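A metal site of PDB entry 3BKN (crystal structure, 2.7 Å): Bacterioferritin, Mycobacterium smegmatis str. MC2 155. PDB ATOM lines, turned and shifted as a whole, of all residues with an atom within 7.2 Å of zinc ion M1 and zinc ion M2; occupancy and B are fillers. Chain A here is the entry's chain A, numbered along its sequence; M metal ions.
The nearest printed residue that does not touch zinc ion M2 is Ile 123 (4.4 Å).
OE1 of Glu 18 is bound to zinc ion M2, at 2.0 Å. Zinc ion M2 is bound by OE1 of Glu 51, 2.0 Å away. The side-chain carboxylate (OE2) of Glu 127 binds zinc ion M2 (2.0 Å). ND1 of His 54 is bound to zinc ion M2.
OE2 of Glu 18 is in hydrogen-bond range of NE2 of Gln 14. OH of Tyr 25 sits close to OE2 of Glu 94 (2.8 Å). NE2 of His 54 is in hydrogen-bond range of OD2 of Asp 126. A ring nitrogen (NE2) of His 130 is in hydrogen-bond range of the side-chain carboxylate (OE1) of Glu 50. NE2 of His 130 sits at hydrogen-bond distance from OE1 of Glu 47, 2.5 Å away.
The side-chain carboxylate (OE1) of Glu 127 binds zinc ion M1, 1.9 Å away. Zinc ion M1 is bound by the side-chain carboxylate (OE2) of Glu 94 (2.0 Å). The side-chain carboxylate (OE2) of Glu 51 is bound to zinc ion M1 (2.0 Å). ND1 of His 130 binds zinc ion M1, 2.1 Å away.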
ATOM      1  N   GLN A  14      10.558 -30.924  32.717  1.00  0.00           N
ATOM      2  CA  GLN A  14      10.469 -29.756  31.863  1.00  0.00           C
ATOM      3  C   GLN A  14       9.331 -28.818  32.294  1.00  0.00           C
ATOM      4  O   GLN A  14       9.498 -27.584  32.291  1.00  0.00           O
ATOM      5  CB  GLN A  14      10.242 -30.142  30.437  1.00  0.00           C
ATOM      6  CG  GLN A  14      10.370 -28.967  29.476  1.00  0.00           C
ATOM      7  CD  GLN A  14      11.713 -28.240  29.610  1.00  0.00           C
ATOM      8  OE1 GLN A  14      12.677 -28.799  30.165  1.00  0.00           O
ATOM      9  NE2 GLN A  14      11.772 -26.994  29.124  1.00  0.00           N
ATOM     10  N   SER A  17      10.437 -26.678  35.031  1.00  0.00           N
ATOM     11  CA  SER A  17      11.245 -25.570  34.455  1.00  0.00           C
ATOM     12  C   SER A  17      10.394 -24.443  33.853  1.00  0.00           C
ATOM     13  O   SER A  17      10.673 -23.266  34.122  1.00  0.00           O
ATOM     14  CB  SER A  17      12.248 -26.032  33.402  1.00  0.00           C
ATOM     15  OG  SER A  17      13.522 -26.216  33.962  1.00  0.00           O
ATOM     16  N   GLU A  18       9.376 -24.779  33.056  1.00  0.00           N
ATOM     17  CA  GLU A  18       8.490 -23.741  32.555  1.00  0.00           C
ATOM     18  C   GLU A  18       7.736 -23.006  33.681  1.00  0.00           C
ATOM     19  O   GLU A  18       7.555 -21.777  33.615  1.00  0.00           O
ATOM     20  CB  GLU A  18       7.458 -24.228  31.541  1.00  0.00           C
ATOM     21  CG  GLU A  18       7.926 -25.156  30.545  1.00  0.00           C
ATOM     22  CD  GLU A  18       8.825 -24.551  29.499  1.00  0.00           C
ATOM     23  OE1 GLU A  18       8.856 -23.315  29.339  1.00  0.00           O
ATOM     24  OE2 GLU A  18       9.458 -25.334  28.792  1.00  0.00           O
ATOM     25  N   ALA A  21      10.201 -20.674  35.017  1.00  0.00           N
ATOM     26  CA  ALA A  21      10.430 -19.564  34.077  1.00  0.00           C
ATOM     27  C   ALA A  21       9.237 -18.575  34.030  1.00  0.00           C
ATOM     28  O   ALA A  21       9.443 -17.385  34.000  1.00  0.00           O
ATOM     29  CB  ALA A  21      10.807 -20.063  32.686  1.00  0.00           C
ATOM     30  N   TYR A  25      10.446 -14.718  34.770  1.00  0.00           N
ATOM     31  CA  TYR A  25      10.199 -13.685  33.756  1.00  0.00           C
ATOM     32  C   TYR A  25       9.114 -12.708  34.170  1.00  0.00           C
ATOM     33  O   TYR A  25       9.297 -11.490  34.104  1.00  0.00           O
ATOM     34  CB  TYR A  25       9.786 -14.318  32.459  1.00  0.00           C
ATOM     35  CG  TYR A  25      10.900 -14.908  31.650  1.00  0.00           C
ATOM     36  CD1 TYR A  25      11.893 -14.073  31.078  1.00  0.00           C
ATOM     37  CD2 TYR A  25      10.944 -16.254  31.378  1.00  0.00           C
ATOM     38  CE1 TYR A  25      12.909 -14.590  30.324  1.00  0.00           C
ATOM     39  CE2 TYR A  25      11.964 -16.800  30.601  1.00  0.00           C
ATOM     40  CZ  TYR A  25      12.929 -15.960  30.065  1.00  0.00           C
ATOM     41  OH  TYR A  25      13.970 -16.461  29.253  1.00  0.00           O
ATOM     42  N   GLU A  47       8.135 -12.775  26.938  1.00  0.00           N
ATOM     43  CA  GLU A  47       8.850 -14.010  27.233  1.00  0.00           C
ATOM     44  C   GLU A  47       8.117 -14.871  28.270  1.00  0.00           C
ATOM     45  O   GLU A  47       8.018 -16.102  28.139  1.00  0.00           O
ATOM     46  CB  GLU A  47      10.298 -13.705  27.632  1.00  0.00           C
ATOM     47  CG  GLU A  47      11.060 -12.879  26.572  1.00  0.00           C
ATOM     48  CD  GLU A  47      11.461 -13.692  25.346  1.00  0.00           C
ATOM     49  OE1 GLU A  47      10.881 -14.778  25.140  1.00  0.00           O
ATOM     50  OE2 GLU A  47      12.367 -13.254  24.596  1.00  0.00           O
ATOM     51  N   GLU A  50       5.226 -16.730  26.611  1.00  0.00           N
ATOM     52  CA  GLU A  50       5.747 -17.846  25.858  1.00  0.00           C
ATOM     53  C   GLU A  50       6.002 -19.007  26.775  1.00  0.00           C
ATOM     54  O   GLU A  50       5.746 -20.127  26.391  1.00  0.00           O
ATOM     55  CB  GLU A  50       7.014 -17.478  25.081  1.00  0.00           C
ATOM     56  CG  GLU A  50       6.842 -17.752  23.555  1.00  0.00           C
ATOM     57  CD  GLU A  50       8.141 -17.795  22.766  1.00  0.00           C
ATOM     58  OE1 GLU A  50       8.646 -16.700  22.372  1.00  0.00           O
ATOM     59  OE2 GLU A  50       8.634 -18.925  22.517  1.00  0.00           O
ATOM     60  N   GLU A  51       6.472 -18.769  28.002  1.00  0.00           N
ATOM     61  CA  GLU A  51       6.626 -19.836  28.953  1.00  0.00           C
ATOM     62  C   GLU A  51       5.305 -20.388  29.377  1.00  0.00           C
ATOM     63  O   GLU A  51       5.170 -21.600  29.519  1.00  0.00           O
ATOM     64  CB  GLU A  51       7.423 -19.443  30.166  1.00  0.00           C
ATOM     65  CG  GLU A  51       8.780 -18.998  29.843  1.00  0.00           C
ATOM     66  CD  GLU A  51       9.593 -19.962  28.981  1.00  0.00           C
ATOM     67  OE1 GLU A  51       9.144 -21.096  28.703  1.00  0.00           O
ATOM     68  OE2 GLU A  51      10.691 -19.568  28.531  1.00  0.00           O
ATOM     69  N   MET A  52       4.316 -19.523  29.606  1.00  0.00           N
ATOM     70  CA  MET A  52       2.974 -19.995  29.924  1.00  0.00           C
ATOM     71  C   MET A  52       2.455 -20.953  28.844  1.00  0.00           C
ATOM     72  O   MET A  52       1.885 -22.007  29.166  1.00  0.00           O
ATOM     73  CB  MET A  52       2.015 -18.840  30.109  1.00  0.00           C
ATOM     74  CG  MET A  52       2.247 -18.044  31.350  1.00  0.00           C
ATOM     75  SD  MET A  52       1.206 -16.556  31.443  1.00  0.00           S
ATOM     76  CE  MET A  52       2.398 -15.409  32.171  1.00  0.00           C
ATOM     77  N   ARG A  53       2.664 -20.611  27.572  1.00  0.00           N
ATOM     78  CA  ARG A  53       2.280 -21.506  26.489  1.00  0.00           C
ATOM     79  C   ARG A  53       3.047 -22.849  26.532  1.00  0.00           C
ATOM     80  O   ARG A  53       2.418 -23.914  26.349  1.00  0.00           O
ATOM     81  CB  ARG A  53       2.369 -20.817  25.142  1.00  0.00           C
ATOM     82  CG  ARG A  53       1.342 -19.707  24.995  1.00  0.00           C
ATOM     83  CD  ARG A  53       1.444 -18.935  23.660  1.00  0.00           C
ATOM     84  NE  ARG A  53       2.541 -17.983  23.722  1.00  0.00           N
ATOM     85  CZ  ARG A  53       3.003 -17.289  22.694  1.00  0.00           C
ATOM     86  NH1 ARG A  53       2.460 -17.417  21.496  1.00  0.00           N
ATOM     87  NH2 ARG A  53       4.021 -16.464  22.869  1.00  0.00           N
ATOM     88  N   HIS A  54       4.346 -22.821  26.809  1.00  0.00           N
ATOM     89  CA  HIS A  54       5.114 -24.035  26.967  1.00  0.00           C
ATOM     90  C   HIS A  54       4.536 -24.963  28.065  1.00  0.00           C
ATOM     91  O   HIS A  54       4.340 -26.177  27.835  1.00  0.00           O
ATOM     92  CB  HIS A  54       6.545 -23.682  27.304  1.00  0.00           C
ATOM     93  CG  HIS A  54       7.288 -23.121  26.158  1.00  0.00           C
ATOM     94  ND1 HIS A  54       8.572 -22.615  26.279  1.00  0.00           N
ATOM     95  CD2 HIS A  54       6.926 -22.944  24.864  1.00  0.00           C
ATOM     96  CE1 HIS A  54       8.982 -22.201  25.094  1.00  0.00           C
ATOM     97  NE2 HIS A  54       7.992 -22.379  24.229  1.00  0.00           N
ATOM     98  N   ALA A  55       4.284 -24.388  29.234  1.00  0.00           N
ATOM     99  CA  ALA A  55       3.650 -25.112  30.314  1.00  0.00           C
ATOM    100  C   ALA A  55       2.355 -25.764  29.828  1.00  0.00           C
ATOM    101  O   ALA A  55       2.103 -26.927  30.114  1.00  0.00           O
ATOM    102  CB  ALA A  55       3.396 -24.204  31.530  1.00  0.00           C
ATOM    103  N   ILE A  58       3.016 -28.801  27.320  1.00  0.00           N
ATOM    104  CA  ILE A  58       3.507 -29.930  28.087  1.00  0.00           C
ATOM    105  C   ILE A  58       2.390 -30.578  28.930  1.00  0.00           C
ATOM    106  O   ILE A  58       2.266 -31.795  28.933  1.00  0.00           O
ATOM    107  CB  ILE A  58       4.753 -29.546  28.948  1.00  0.00           C
ATOM    108  CG1 ILE A  58       5.992 -29.304  28.070  1.00  0.00           C
ATOM    109  CG2 ILE A  58       5.092 -30.645  29.988  1.00  0.00           C
ATOM    110  CD1 ILE A  58       7.041 -28.330  28.723  1.00  0.00           C
ATOM    111  N   ASP A  90      17.863 -15.201  33.860  1.00  0.00           N
ATOM    112  CA  ASP A  90      17.013 -15.861  32.856  1.00  0.00           C
ATOM    113  C   ASP A  90      17.851 -16.728  31.898  1.00  0.00           C
ATOM    114  O   ASP A  90      17.449 -17.811  31.482  1.00  0.00           O
ATOM    115  CB  ASP A  90      16.140 -14.837  32.127  1.00  0.00           C
ATOM    116  CG  ASP A  90      15.121 -14.142  33.072  1.00  0.00           C
ATOM    117  OD1 ASP A  90      14.609 -14.832  34.001  1.00  0.00           O
ATOM    118  OD2 ASP A  90      14.849 -12.906  32.894  1.00  0.00           O
ATOM    119  N   ILE A  93      18.434 -20.212  33.604  1.00  0.00           N
ATOM    120  CA  ILE A  93      17.443 -21.255  33.406  1.00  0.00           C
ATOM    121  C   ILE A  93      17.239 -21.748  31.965  1.00  0.00           C
ATOM    122  O   ILE A  93      16.843 -22.905  31.762  1.00  0.00           O
ATOM    123  CB  ILE A  93      16.075 -21.039  34.073  1.00  0.00           C
ATOM    124  CG1 ILE A  93      15.537 -19.674  33.839  1.00  0.00           C
ATOM    125  CG2 ILE A  93      16.117 -21.405  35.591  1.00  0.00           C
ATOM    126  CD1 ILE A  93      14.247 -19.528  34.616  1.00  0.00           C
ATOM    127  N   GLU A  94      17.478 -20.889  30.980  1.00  0.00           N
ATOM    128  CA  GLU A  94      17.383 -21.355  29.607  1.00  0.00           C
ATOM    129  C   GLU A  94      18.454 -22.389  29.348  1.00  0.00           C
ATOM    130  O   GLU A  94      18.172 -23.397  28.702  1.00  0.00           O
ATOM    131  CB  GLU A  94      17.420 -20.205  28.614  1.00  0.00           C
ATOM    132  CG  GLU A  94      16.258 -19.245  28.754  1.00  0.00           C
ATOM    133  CD  GLU A  94      14.922 -19.845  28.341  1.00  0.00           C
ATOM    134  OE1 GLU A  94      14.837 -21.038  27.955  1.00  0.00           O
ATOM    135  OE2 GLU A  94      13.921 -19.110  28.406  1.00  0.00           O
ATOM    136  N   VAL A  97      17.480 -25.688  30.632  1.00  0.00           N
ATOM    137  CA  VAL A  97      16.559 -26.331  29.718  1.00  0.00           C
ATOM    138  C   VAL A  97      17.304 -27.068  28.597  1.00  0.00           C
ATOM    139  O   VAL A  97      17.019 -28.236  28.341  1.00  0.00           O
ATOM    140  CB  VAL A  97      15.488 -25.354  29.256  1.00  0.00           C
ATOM    141  CG1 VAL A  97      14.703 -25.939  28.093  1.00  0.00           C
ATOM    142  CG2 VAL A  97      14.563 -25.044  30.436  1.00  0.00           C
ATOM    143  N   ILE A 123       9.974 -26.849  21.733  1.00  0.00           N
ATOM    144  CA  ILE A 123      10.325 -26.083  22.885  1.00  0.00           C
ATOM    145  C   ILE A 123      11.815 -25.692  22.856  1.00  0.00           C
ATOM    146  O   ILE A 123      12.162 -24.513  23.036  1.00  0.00           O
ATOM    147  CB  ILE A 123       9.845 -26.764  24.176  1.00  0.00           C
ATOM    148  CG1 ILE A 123       8.338 -26.481  24.338  1.00  0.00           C
ATOM    149  CG2 ILE A 123      10.594 -26.268  25.396  1.00  0.00           C
ATOM    150  CD1 ILE A 123       7.667 -27.469  25.140  1.00  0.00           C
ATOM    151  N   LEU A 124      12.676 -26.659  22.562  1.00  0.00           N
ATOM    152  CA  LEU A 124      14.114 -26.418  22.491  1.00  0.00           C
ATOM    153  C   LEU A 124      14.437 -25.272  21.547  1.00  0.00           C
ATOM    154  O   LEU A 124      15.189 -24.353  21.903  1.00  0.00           O
ATOM    155  CB  LEU A 124      14.897 -27.680  22.097  1.00  0.00           C
ATOM    156  CG  LEU A 124      16.433 -27.647  22.057  1.00  0.00           C
ATOM    157  CD1 LEU A 124      17.061 -27.049  23.319  1.00  0.00           C
ATOM    158  CD2 LEU A 124      17.014 -29.005  21.791  1.00  0.00           C
ATOM    159  N   ASP A 126      12.472 -22.772  20.579  1.00  0.00           N
ATOM    160  CA  ASP A 126      12.056 -21.546  21.241  1.00  0.00           C
ATOM    161  C   ASP A 126      13.086 -21.152  22.330  1.00  0.00           C
ATOM    162  O   ASP A 126      13.546 -20.021  22.358  1.00  0.00           O
ATOM    163  CB  ASP A 126      10.630 -21.632  21.822  1.00  0.00           C
ATOM    164  CG  ASP A 126       9.520 -21.846  20.728  1.00  0.00           C
ATOM    165  OD1 ASP A 126       9.767 -21.975  19.500  1.00  0.00           O
ATOM    166  OD2 ASP A 126       8.341 -21.908  21.108  1.00  0.00           O
ATOM    167  N   GLU A 127      13.510 -22.071  23.172  1.00  0.00           N
ATOM    168  CA  GLU A 127      14.482 -21.655  24.198  1.00  0.00           C
ATOM    169  C   GLU A 127      15.828 -21.248  23.637  1.00  0.00           C
ATOM    170  O   GLU A 127      16.493 -20.419  24.241  1.00  0.00           O
ATOM    171  CB  GLU A 127      14.625 -22.666  25.351  1.00  0.00           C
ATOM    172  CG  GLU A 127      13.381 -23.377  25.736  1.00  0.00           C
ATOM    173  CD  GLU A 127      12.441 -22.556  26.568  1.00  0.00           C
ATOM    174  OE1 GLU A 127      12.336 -21.341  26.310  1.00  0.00           O
ATOM    175  OE2 GLU A 127      11.768 -23.120  27.468  1.00  0.00           O
ATOM    176  N   GLU A 128      16.243 -21.796  22.510  1.00  0.00           N
ATOM    177  CA  GLU A 128      17.527 -21.399  21.913  1.00  0.00           C
ATOM    178  C   GLU A 128      17.386 -19.964  21.435  1.00  0.00           C
ATOM    179  O   GLU A 128      18.306 -19.174  21.560  1.00  0.00           O
ATOM    180  CB  GLU A 128      17.959 -22.320  20.778  1.00  0.00           C
ATOM    181  CG  GLU A 128      18.420 -23.691  21.218  1.00  0.00           C
ATOM    182  CD  GLU A 128      19.017 -24.574  20.089  1.00  0.00           C
ATOM    183  OE1 GLU A 128      19.703 -24.028  19.184  1.00  0.00           O
ATOM    184  OE2 GLU A 128      18.848 -25.820  20.104  1.00  0.00           O
ATOM    185  N   THR A 129      16.223 -19.601  20.955  1.00  0.00           N
ATOM    186  CA  THR A 129      15.983 -18.224  20.574  1.00  0.00           C
ATOM    187  C   THR A 129      16.025 -17.236  21.774  1.00  0.00           C
ATOM    188  O   THR A 129      16.577 -16.138  21.636  1.00  0.00           O
ATOM    189  CB  THR A 129      14.708 -18.136  19.709  1.00  0.00           C
ATOM    190  OG1 THR A 129      15.012 -18.741  18.450  1.00  0.00           O
ATOM    191  CG2 THR A 129      14.249 -16.697  19.476  1.00  0.00           C
ATOM    192  N   HIS A 130      15.482 -17.642  22.923  1.00  0.00           N
ATOM    193  CA  HIS A 130      15.558 -16.831  24.129  1.00  0.00           C
ATOM    194  C   HIS A 130      17.018 -16.686  24.498  1.00  0.00           C
ATOM    195  O   HIS A 130      17.455 -15.585  24.785  1.00  0.00           O
ATOM    196  CB  HIS A 130      14.776 -17.409  25.328  1.00  0.00           C
ATOM    197  CG  HIS A 130      13.269 -17.393  25.172  1.00  0.00           C
ATOM    198  ND1 HIS A 130      12.430 -17.996  26.088  1.00  0.00           N
ATOM    199  CD2 HIS A 130      12.466 -16.890  24.195  1.00  0.00           C
ATOM    200  CE1 HIS A 130      11.171 -17.853  25.703  1.00  0.00           C
ATOM    201  NE2 HIS A 130      11.159 -17.195  24.553  1.00  0.00           N
ATOM    202  N   ILE A 131      17.783 -17.765  24.448  1.00  0.00           N
ATOM    203  CA  ILE A 131      19.215 -17.694  24.758  1.00  0.00           C
ATOM    204  C   ILE A 131      19.931 -16.727  23.857  1.00  0.00           C
ATOM    205  O   ILE A 131      20.739 -15.963  24.317  1.00  0.00           O
ATOM    206  CB  ILE A 131      19.916 -19.098  24.692  1.00  0.00           C
ATOM    207  CG1 ILE A 131      19.426 -19.982  25.846  1.00  0.00           C
ATOM    208  CG2 ILE A 131      21.449 -18.965  24.726  1.00  0.00           C
ATOM    209  CD1 ILE A 131      19.607 -21.447  25.603  1.00  0.00           C
ATOM    210  N   LEU A 134      19.080 -13.147  24.908  1.00  0.00           N
ATOM    211  CA  LEU A 134      19.685 -12.848  26.199  1.00  0.00           C
ATOM    212  C   LEU A 134      21.162 -12.620  26.087  1.00  0.00           C
ATOM    213  O   LEU A 134      21.691 -11.651  26.648  1.00  0.00           O
ATOM    214  CB  LEU A 134      19.454 -13.979  27.174  1.00  0.00           C
ATOM    215  CG  LEU A 134      18.001 -14.199  27.631  1.00  0.00           C
ATOM    216  CD1 LEU A 134      17.865 -15.532  28.316  1.00  0.00           C
ATOM    217  CD2 LEU A 134      17.562 -13.062  28.533  1.00  0.00           C
HETATM  218 ZN    ZN M   1      12.330 -19.729  27.338  1.00  0.00          ZN
HETATM  219 ZN    ZN M   2       9.891 -22.668  27.811  1.00  0.00          ZN
